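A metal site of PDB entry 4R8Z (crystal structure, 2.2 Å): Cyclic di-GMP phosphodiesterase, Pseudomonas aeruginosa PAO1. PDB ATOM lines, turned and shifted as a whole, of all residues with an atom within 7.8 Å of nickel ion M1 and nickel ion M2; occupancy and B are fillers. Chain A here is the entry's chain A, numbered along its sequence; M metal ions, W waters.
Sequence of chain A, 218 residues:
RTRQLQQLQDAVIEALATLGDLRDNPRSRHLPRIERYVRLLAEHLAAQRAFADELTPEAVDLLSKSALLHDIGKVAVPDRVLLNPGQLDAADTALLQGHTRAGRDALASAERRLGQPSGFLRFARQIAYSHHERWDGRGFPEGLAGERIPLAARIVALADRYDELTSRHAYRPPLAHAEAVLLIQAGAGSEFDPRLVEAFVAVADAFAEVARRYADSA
ND1 of His 70 sits at hydrogen-bond distance from O of Ala 67 (3.0 Å). OD2 of Asp 71 sits close to NZ of Lys 74 (3.2 Å). The backbone carbonyl oxygen of Ile 127 lies within hydrogen-bond range of a ring nitrogen (ND1) of His 131, 3.0 Å away. The backbone carbonyl oxygen (O) of His 132 sits at hydrogen-bond distance from the backbone NH (N) of Phe 140 (3.3 Å). A ring nitrogen (ND1) of His 30 lies within hydrogen-bond range of the side-chain carboxylate (OD2) of Asp 163, 2.8 Å away. ND1 of His 131 sits at hydrogen-bond distance from O of Ala 128, at 3.2 Å. ND1 of His 99 is in hydrogen-bond range of O of Leu 96, at 2.9 Å.
Four residues have an atom within 4 Å of nickel ion M1: Asp 71, His 99, His 131 and His 132.
Of the 25 residues printed, 3 come within 4 Å of nickel ion M2.
Nickel ion M1 is bound by water W3 (1.9 Å), the side-chain carboxylate of Asp 71 (2.0 Å), a ring nitrogen (NE2) of His 131 (2.0 Å), a ring nitrogen (NE2) of His 132 (2.1 Å), water W2 (2.1 Å) and a ring nitrogen (NE2) of His 99 (2.1 Å). Nickel ion M1 has six donor atoms within binding distance.
Nickel ion M2 is bound by water W1 (2.0 Å). Nickel ion M2 is bound by water W4 (2.0 Å). Nickel ion M2 is bound by NE2 of His 70, at 2.0 Å. Nickel ion M2 is bound by water W5 (2.1 Å). Nickel ion M2 is bound by OD2 of Asp 71, 2.1 Å away. NE2 of His 30 binds nickel ion M2 (2.1 Å). Nickel ion M2 has six donor atoms within binding distance.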
ATOM      1  N   ASP A  21      20.481   2.833   1.324  1.00  0.00           N
ATOM      2  CA  ASP A  21      21.035   3.212  -0.002  1.00  0.00           C
ATOM      3  C   ASP A  21      21.519   1.954  -0.735  1.00  0.00           C
ATOM      4  O   ASP A  21      22.019   2.029  -1.850  1.00  0.00           O
ATOM      5  CB  ASP A  21      22.236   4.148   0.199  1.00  0.00           C
ATOM      6  CG  ASP A  21      21.908   5.680   0.043  1.00  0.00           C
ATOM      7  OD1 ASP A  21      20.714   6.062  -0.142  1.00  0.00           O
ATOM      8  OD2 ASP A  21      22.897   6.510   0.097  1.00  0.00           O
ATOM      9  N   ASP A  24      20.056   1.011  -4.453  1.00  0.00           N
ATOM     10  CA  ASP A  24      20.351   1.793  -5.640  1.00  0.00           C
ATOM     11  C   ASP A  24      21.654   2.545  -5.603  1.00  0.00           C
ATOM     12  O   ASP A  24      21.964   3.187  -6.588  1.00  0.00           O
ATOM     13  CB  ASP A  24      19.227   2.757  -5.985  1.00  0.00           C
ATOM     14  CG  ASP A  24      19.208   3.971  -5.060  1.00  0.00           C
ATOM     15  OD1 ASP A  24      19.661   3.872  -3.898  1.00  0.00           O
ATOM     16  OD2 ASP A  24      18.718   5.029  -5.496  1.00  0.00           O
ATOM     17  N   ASN A  25      22.418   2.491  -4.508  1.00  0.00           N
ATOM     18  CA  ASN A  25      23.621   3.290  -4.367  1.00  0.00           C
ATOM     19  C   ASN A  25      24.695   2.674  -3.421  1.00  0.00           C
ATOM     20  O   ASN A  25      25.077   3.301  -2.437  1.00  0.00           O
ATOM     21  CB  ASN A  25      23.228   4.698  -3.903  1.00  0.00           C
ATOM     22  CG  ASN A  25      24.417   5.661  -3.921  1.00  0.00           C
ATOM     23  OD1 ASN A  25      25.233   5.631  -4.831  1.00  0.00           O
ATOM     24  ND2 ASN A  25      24.550   6.467  -2.890  1.00  0.00           N
ATOM     25  N   HIS A  30      28.063   9.094  -0.489  1.00  0.00           N
ATOM     26  CA  HIS A  30      26.995  10.078  -0.632  1.00  0.00           C
ATOM     27  C   HIS A  30      26.579  10.728   0.699  1.00  0.00           C
ATOM     28  O   HIS A  30      26.426  11.933   0.786  1.00  0.00           O
ATOM     29  CB  HIS A  30      25.825   9.330  -1.303  1.00  0.00           C
ATOM     30  CG  HIS A  30      24.529  10.062  -1.428  1.00  0.00           C
ATOM     31  ND1 HIS A  30      24.427  11.287  -2.036  1.00  0.00           N
ATOM     32  CD2 HIS A  30      23.249   9.711  -1.070  1.00  0.00           C
ATOM     33  CE1 HIS A  30      23.143  11.671  -2.058  1.00  0.00           C
ATOM     34  NE2 HIS A  30      22.401  10.717  -1.495  1.00  0.00           N
ATOM     35  N   LEU A  31      26.396   9.929   1.726  1.00  0.00           N
ATOM     36  CA  LEU A  31      25.781  10.455   2.918  1.00  0.00           C
ATOM     37  C   LEU A  31      26.671  11.390   3.746  1.00  0.00           C
ATOM     38  O   LEU A  31      26.255  12.477   4.125  1.00  0.00           O
ATOM     39  CB  LEU A  31      25.238   9.348   3.814  1.00  0.00           C
ATOM     40  CG  LEU A  31      24.167   8.548   3.115  1.00  0.00           C
ATOM     41  CD1 LEU A  31      23.696   7.342   3.910  1.00  0.00           C
ATOM     42  CD2 LEU A  31      22.985   9.403   2.684  1.00  0.00           C
ATOM     43  N   ILE A  34      26.822  14.648   1.634  1.00  0.00           N
ATOM     44  CA  ILE A  34      25.616  15.470   1.696  1.00  0.00           C
ATOM     45  C   ILE A  34      25.526  16.222   2.993  1.00  0.00           C
ATOM     46  O   ILE A  34      25.217  17.430   3.044  1.00  0.00           O
ATOM     47  CB  ILE A  34      24.285  14.674   1.549  1.00  0.00           C
ATOM     48  CG1 ILE A  34      24.142  14.082   0.173  1.00  0.00           C
ATOM     49  CG2 ILE A  34      23.084  15.596   1.620  1.00  0.00           C
ATOM     50  CD1 ILE A  34      24.267  15.040  -0.985  1.00  0.00           C
ATOM     51  N   ALA A  67      19.647  15.565   7.253  1.00  0.00           N
ATOM     52  CA  ALA A  67      19.742  15.411   5.791  1.00  0.00           C
ATOM     53  C   ALA A  67      20.116  14.013   5.373  1.00  0.00           C
ATOM     54  O   ALA A  67      19.765  13.586   4.294  1.00  0.00           O
ATOM     55  CB  ALA A  67      20.719  16.416   5.224  1.00  0.00           C
ATOM     56  N   LEU A  68      20.746  13.267   6.267  1.00  0.00           N
ATOM     57  CA  LEU A  68      21.077  11.868   5.992  1.00  0.00           C
ATOM     58  C   LEU A  68      19.873  10.964   5.641  1.00  0.00           C
ATOM     59  O   LEU A  68      20.043   9.920   4.959  1.00  0.00           O
ATOM     60  CB  LEU A  68      21.749  11.243   7.209  1.00  0.00           C
ATOM     61  CG  LEU A  68      23.124  11.729   7.620  1.00  0.00           C
ATOM     62  CD1 LEU A  68      23.615  10.972   8.866  1.00  0.00           C
ATOM     63  CD2 LEU A  68      24.129  11.490   6.553  1.00  0.00           C
ATOM     64  N   LEU A  69      18.703  11.327   6.121  1.00  0.00           N
ATOM     65  CA  LEU A  69      17.514  10.494   5.914  1.00  0.00           C
ATOM     66  C   LEU A  69      16.710  10.836   4.640  1.00  0.00           C
ATOM     67  O   LEU A  69      15.595  10.300   4.472  1.00  0.00           O
ATOM     68  CB  LEU A  69      16.607  10.616   7.149  1.00  0.00           C
ATOM     69  CG  LEU A  69      17.254  10.067   8.409  1.00  0.00           C
ATOM     70  CD1 LEU A  69      16.463  10.374   9.658  1.00  0.00           C
ATOM     71  CD2 LEU A  69      17.421   8.533   8.293  1.00  0.00           C
ATOM     72  N   HIS A  70      17.238  11.701   3.776  1.00  0.00           N
ATOM     73  CA  HIS A  70      16.434  12.249   2.663  1.00  0.00           C
ATOM     74  C   HIS A  70      15.804  11.144   1.864  1.00  0.00           C
ATOM     75  O   HIS A  70      14.642  11.266   1.472  1.00  0.00           O
ATOM     76  CB  HIS A  70      17.256  13.257   1.808  1.00  0.00           C
ATOM     77  CG  HIS A  70      18.387  12.667   1.022  1.00  0.00           C
ATOM     78  ND1 HIS A  70      19.628  12.399   1.582  1.00  0.00           N
ATOM     79  CD2 HIS A  70      18.465  12.256  -0.266  1.00  0.00           C
ATOM     80  CE1 HIS A  70      20.406  11.844   0.668  1.00  0.00           C
ATOM     81  NE2 HIS A  70      19.694  11.690  -0.444  1.00  0.00           N
ATOM     82  N   ASP A  71      16.506  10.066   1.614  1.00  0.00           N
ATOM     83  CA  ASP A  71      16.067   9.053   0.630  1.00  0.00           C
ATOM     84  C   ASP A  71      15.685   7.718   1.303  1.00  0.00           C
ATOM     85  O   ASP A  71      15.661   6.656   0.668  1.00  0.00           O
ATOM     86  CB  ASP A  71      17.205   8.759  -0.424  1.00  0.00           C
ATOM     87  CG  ASP A  71      17.230   9.753  -1.665  1.00  0.00           C
ATOM     88  OD1 ASP A  71      16.113  10.297  -2.052  1.00  0.00           O
ATOM     89  OD2 ASP A  71      18.389   9.958  -2.191  1.00  0.00           O
ATOM     90  N   ILE A  72      15.423   7.731   2.582  1.00  0.00           N
ATOM     91  CA  ILE A  72      15.096   6.408   3.234  1.00  0.00           C
ATOM     92  C   ILE A  72      13.801   5.776   2.738  1.00  0.00           C
ATOM     93  O   ILE A  72      13.613   4.579   2.848  1.00  0.00           O
ATOM     94  CB  ILE A  72      14.818   6.572   4.747  1.00  0.00           C
ATOM     95  CG1 ILE A  72      13.777   7.644   4.939  1.00  0.00           C
ATOM     96  CG2 ILE A  72      16.096   6.798   5.485  1.00  0.00           C
ATOM     97  CD1 ILE A  72      13.472   7.962   6.363  1.00  0.00           C
ATOM     98  N   LYS A  74      13.072   5.085  -0.245  1.00  0.00           N
ATOM     99  CA  LYS A  74      13.237   4.312  -1.464  1.00  0.00           C
ATOM    100  C   LYS A  74      12.870   2.855  -1.390  1.00  0.00           C
ATOM    101  O   LYS A  74      12.731   2.228  -2.433  1.00  0.00           O
ATOM    102  CB  LYS A  74      14.649   4.409  -1.973  1.00  0.00           C
ATOM    103  CG  LYS A  74      14.767   5.642  -2.867  1.00  0.00           C
ATOM    104  CD  LYS A  74      16.168   5.945  -3.213  1.00  0.00           C
ATOM    105  CE  LYS A  74      16.199   7.149  -4.165  1.00  0.00           C
ATOM    106  NZ  LYS A  74      17.643   7.588  -4.221  1.00  0.00           N
ATOM    107  N   LEU A  96       8.651   5.949  -8.420  1.00  0.00           N
ATOM    108  CA  LEU A  96       9.916   6.532  -8.042  1.00  0.00           C
ATOM    109  C   LEU A  96       9.774   7.804  -7.172  1.00  0.00           C
ATOM    110  O   LEU A  96      10.429   7.923  -6.121  1.00  0.00           O
ATOM    111  CB  LEU A  96      10.728   6.810  -9.297  1.00  0.00           C
ATOM    112  CG  LEU A  96      12.097   7.481  -9.118  1.00  0.00           C
ATOM    113  CD1 LEU A  96      13.031   6.571  -8.328  1.00  0.00           C
ATOM    114  CD2 LEU A  96      12.765   7.874 -10.444  1.00  0.00           C
ATOM    115  N   GLN A  97       8.870   8.685  -7.567  1.00  0.00           N
ATOM    116  CA  GLN A  97       8.545   9.877  -6.807  1.00  0.00           C
ATOM    117  C   GLN A  97       7.993   9.611  -5.407  1.00  0.00           C
ATOM    118  O   GLN A  97       8.230  10.408  -4.455  1.00  0.00           O
ATOM    119  CB  GLN A  97       7.600  10.779  -7.564  1.00  0.00           C
ATOM    120  CG  GLN A  97       8.245  11.283  -8.869  1.00  0.00           C
ATOM    121  CD  GLN A  97       7.322  12.175  -9.697  1.00  0.00           C
ATOM    122  OE1 GLN A  97       6.146  12.370  -9.389  1.00  0.00           O
ATOM    123  NE2 GLN A  97       7.859  12.724 -10.752  1.00  0.00           N
ATOM    124  N   HIS A  99       9.072   7.784  -3.202  1.00  0.00           N
ATOM    125  CA  HIS A  99      10.089   7.756  -2.124  1.00  0.00           C
ATOM    126  C   HIS A  99       9.940   8.900  -1.125  1.00  0.00           C
ATOM    127  O   HIS A  99      10.223   8.733   0.048  1.00  0.00           O
ATOM    128  CB  HIS A  99      11.500   7.588  -2.626  1.00  0.00           C
ATOM    129  CG  HIS A  99      12.199   8.856  -3.047  1.00  0.00           C
ATOM    130  ND1 HIS A  99      12.016   9.433  -4.281  1.00  0.00           N
ATOM    131  CD2 HIS A  99      13.193   9.553  -2.458  1.00  0.00           C
ATOM    132  CE1 HIS A  99      12.836  10.476  -4.402  1.00  0.00           C
ATOM    133  NE2 HIS A  99      13.603  10.533  -3.340  1.00  0.00           N
ATOM    134  N   THR A 100       9.433  10.046  -1.564  1.00  0.00           N
ATOM    135  CA  THR A 100       9.345  11.235  -0.739  1.00  0.00           C
ATOM    136  C   THR A 100       8.206  11.017   0.257  1.00  0.00           C
ATOM    137  O   THR A 100       8.406  11.199   1.440  1.00  0.00           O
ATOM    138  CB  THR A 100       9.060  12.499  -1.579  1.00  0.00           C
ATOM    139  OG1 THR A 100       7.951  12.243  -2.460  1.00  0.00           O
ATOM    140  CG2 THR A 100      10.285  12.778  -2.479  1.00  0.00           C
ATOM    141  N   ILE A 127      12.676  17.458   4.864  1.00  0.00           N
ATOM    142  CA  ILE A 127      13.621  17.096   3.851  1.00  0.00           C
ATOM    143  C   ILE A 127      13.165  15.886   3.087  1.00  0.00           C
ATOM    144  O   ILE A 127      13.225  15.832   1.859  1.00  0.00           O
ATOM    145  CB  ILE A 127      14.984  16.877   4.447  1.00  0.00           C
ATOM    146  CG1 ILE A 127      15.583  18.237   4.796  1.00  0.00           C
ATOM    147  CG2 ILE A 127      15.910  16.148   3.496  1.00  0.00           C
ATOM    148  CD1 ILE A 127      16.662  18.155   5.856  1.00  0.00           C
ATOM    149  N   ALA A 128      12.764  14.856   3.770  1.00  0.00           N
ATOM    150  CA  ALA A 128      12.444  13.659   3.013  1.00  0.00           C
ATOM    151  C   ALA A 128      11.322  13.926   2.030  1.00  0.00           C
ATOM    152  O   ALA A 128      11.270  13.362   0.939  1.00  0.00           O
ATOM    153  CB  ALA A 128      12.046  12.543   3.940  1.00  0.00           C
ATOM    154  N   HIS A 131      12.576  17.354  -0.669  1.00  0.00           N
ATOM    155  CA  HIS A 131      13.912  17.499  -1.250  1.00  0.00           C
ATOM    156  C   HIS A 131      13.984  17.485  -2.829  1.00  0.00           C
ATOM    157  O   HIS A 131      15.010  17.816  -3.388  1.00  0.00           O
ATOM    158  CB  HIS A 131      14.927  16.537  -0.628  1.00  0.00           C
ATOM    159  CG  HIS A 131      14.855  15.105  -1.048  1.00  0.00           C
ATOM    160  ND1 HIS A 131      13.980  14.193  -0.503  1.00  0.00           N
ATOM    161  CD2 HIS A 131      15.589  14.404  -1.934  1.00  0.00           C
ATOM    162  CE1 HIS A 131      14.141  13.015  -1.065  1.00  0.00           C
ATOM    163  NE2 HIS A 131      15.092  13.118  -1.982  1.00  0.00           N
ATOM    164  N   HIS A 132      12.901  17.117  -3.503  1.00  0.00           N
ATOM    165  CA  HIS A 132      12.847  17.166  -4.959  1.00  0.00           C
ATOM    166  C   HIS A 132      11.830  18.243  -5.375  1.00  0.00           C
ATOM    167  O   HIS A 132      11.460  18.295  -6.551  1.00  0.00           O
ATOM    168  CB  HIS A 132      12.448  15.845  -5.548  1.00  0.00           C
ATOM    169  CG  HIS A 132      13.434  14.740  -5.359  1.00  0.00           C
ATOM    170  ND1 HIS A 132      14.563  14.588  -6.114  1.00  0.00           N
ATOM    171  CD2 HIS A 132      13.433  13.701  -4.480  1.00  0.00           C
ATOM    172  CE1 HIS A 132      15.222  13.502  -5.713  1.00  0.00           C
ATOM    173  NE2 HIS A 132      14.583  12.988  -4.679  1.00  0.00           N
ATOM    174  N   PHE A 140       8.305  17.724  -7.450  1.00  0.00           N
ATOM    175  CA  PHE A 140       7.374  16.799  -6.884  1.00  0.00           C
ATOM    176  C   PHE A 140       7.707  16.595  -5.401  1.00  0.00           C
ATOM    177  O   PHE A 140       8.839  16.870  -5.017  1.00  0.00           O
ATOM    178  CB  PHE A 140       7.454  15.516  -7.685  1.00  0.00           C
ATOM    179  CG  PHE A 140       8.787  14.792  -7.646  1.00  0.00           C
ATOM    180  CD1 PHE A 140       9.101  13.909  -6.616  1.00  0.00           C
ATOM    181  CD2 PHE A 140       9.702  14.941  -8.714  1.00  0.00           C
ATOM    182  CE1 PHE A 140      10.316  13.228  -6.575  1.00  0.00           C
ATOM    183  CE2 PHE A 140      10.902  14.219  -8.741  1.00  0.00           C
ATOM    184  CZ  PHE A 140      11.212  13.363  -7.642  1.00  0.00           C
ATOM    185  N   VAL A 156      18.898  21.155   0.905  1.00  0.00           N
ATOM    186  CA  VAL A 156      19.223  19.817   0.510  1.00  0.00           C
ATOM    187  C   VAL A 156      19.117  19.590  -0.979  1.00  0.00           C
ATOM    188  O   VAL A 156      19.966  18.893  -1.570  1.00  0.00           O
ATOM    189  CB  VAL A 156      18.409  18.760   1.273  1.00  0.00           C
ATOM    190  CG1 VAL A 156      18.667  17.347   0.773  1.00  0.00           C
ATOM    191  CG2 VAL A 156      18.774  18.808   2.714  1.00  0.00           C
ATOM    192  N   ASP A 160      22.171  18.005  -2.973  1.00  0.00           N
ATOM    193  CA  ASP A 160      21.929  16.692  -3.593  1.00  0.00           C
ATOM    194  C   ASP A 160      22.276  16.725  -5.075  1.00  0.00           C
ATOM    195  O   ASP A 160      22.858  15.792  -5.602  1.00  0.00           O
ATOM    196  CB  ASP A 160      20.472  16.352  -3.415  1.00  0.00           C
ATOM    197  CG  ASP A 160      20.119  14.879  -3.586  1.00  0.00           C
ATOM    198  OD1 ASP A 160      20.961  13.946  -3.384  1.00  0.00           O
ATOM    199  OD2 ASP A 160      18.859  14.634  -3.862  1.00  0.00           O
ATOM    200  N   ASP A 163      26.104  16.879  -5.426  1.00  0.00           N
ATOM    201  CA  ASP A 163      26.657  15.568  -5.197  1.00  0.00           C
ATOM    202  C   ASP A 163      26.432  14.587  -6.337  1.00  0.00           C
ATOM    203  O   ASP A 163      27.335  13.834  -6.716  1.00  0.00           O
ATOM    204  CB  ASP A 163      26.103  14.896  -3.978  1.00  0.00           C
ATOM    205  CG  ASP A 163      26.986  13.692  -3.548  1.00  0.00           C
ATOM    206  OD1 ASP A 163      28.223  13.913  -3.324  1.00  0.00           O
ATOM    207  OD2 ASP A 163      26.489  12.560  -3.486  1.00  0.00           O
HETATM  208 NI    NI M   1      15.349  11.630  -3.346  1.00  0.00          NI
HETATM  209 NI    NI M   2      20.366  10.231  -1.698  1.00  0.00          NI
HETATM  210  O   HOH W   1      20.785   8.753  -2.965  1.00  0.00           O
HETATM  211  O   HOH W   2      17.293  12.265  -3.572  1.00  0.00           O
HETATM  212  O   HOH W   3      16.019  10.419  -4.657  1.00  0.00           O
HETATM  213  O   HOH W   4      20.412  11.548  -3.227  1.00  0.00           O
HETATM  214  O   HOH W   5      20.435   8.850  -0.183  1.00  0.00           O
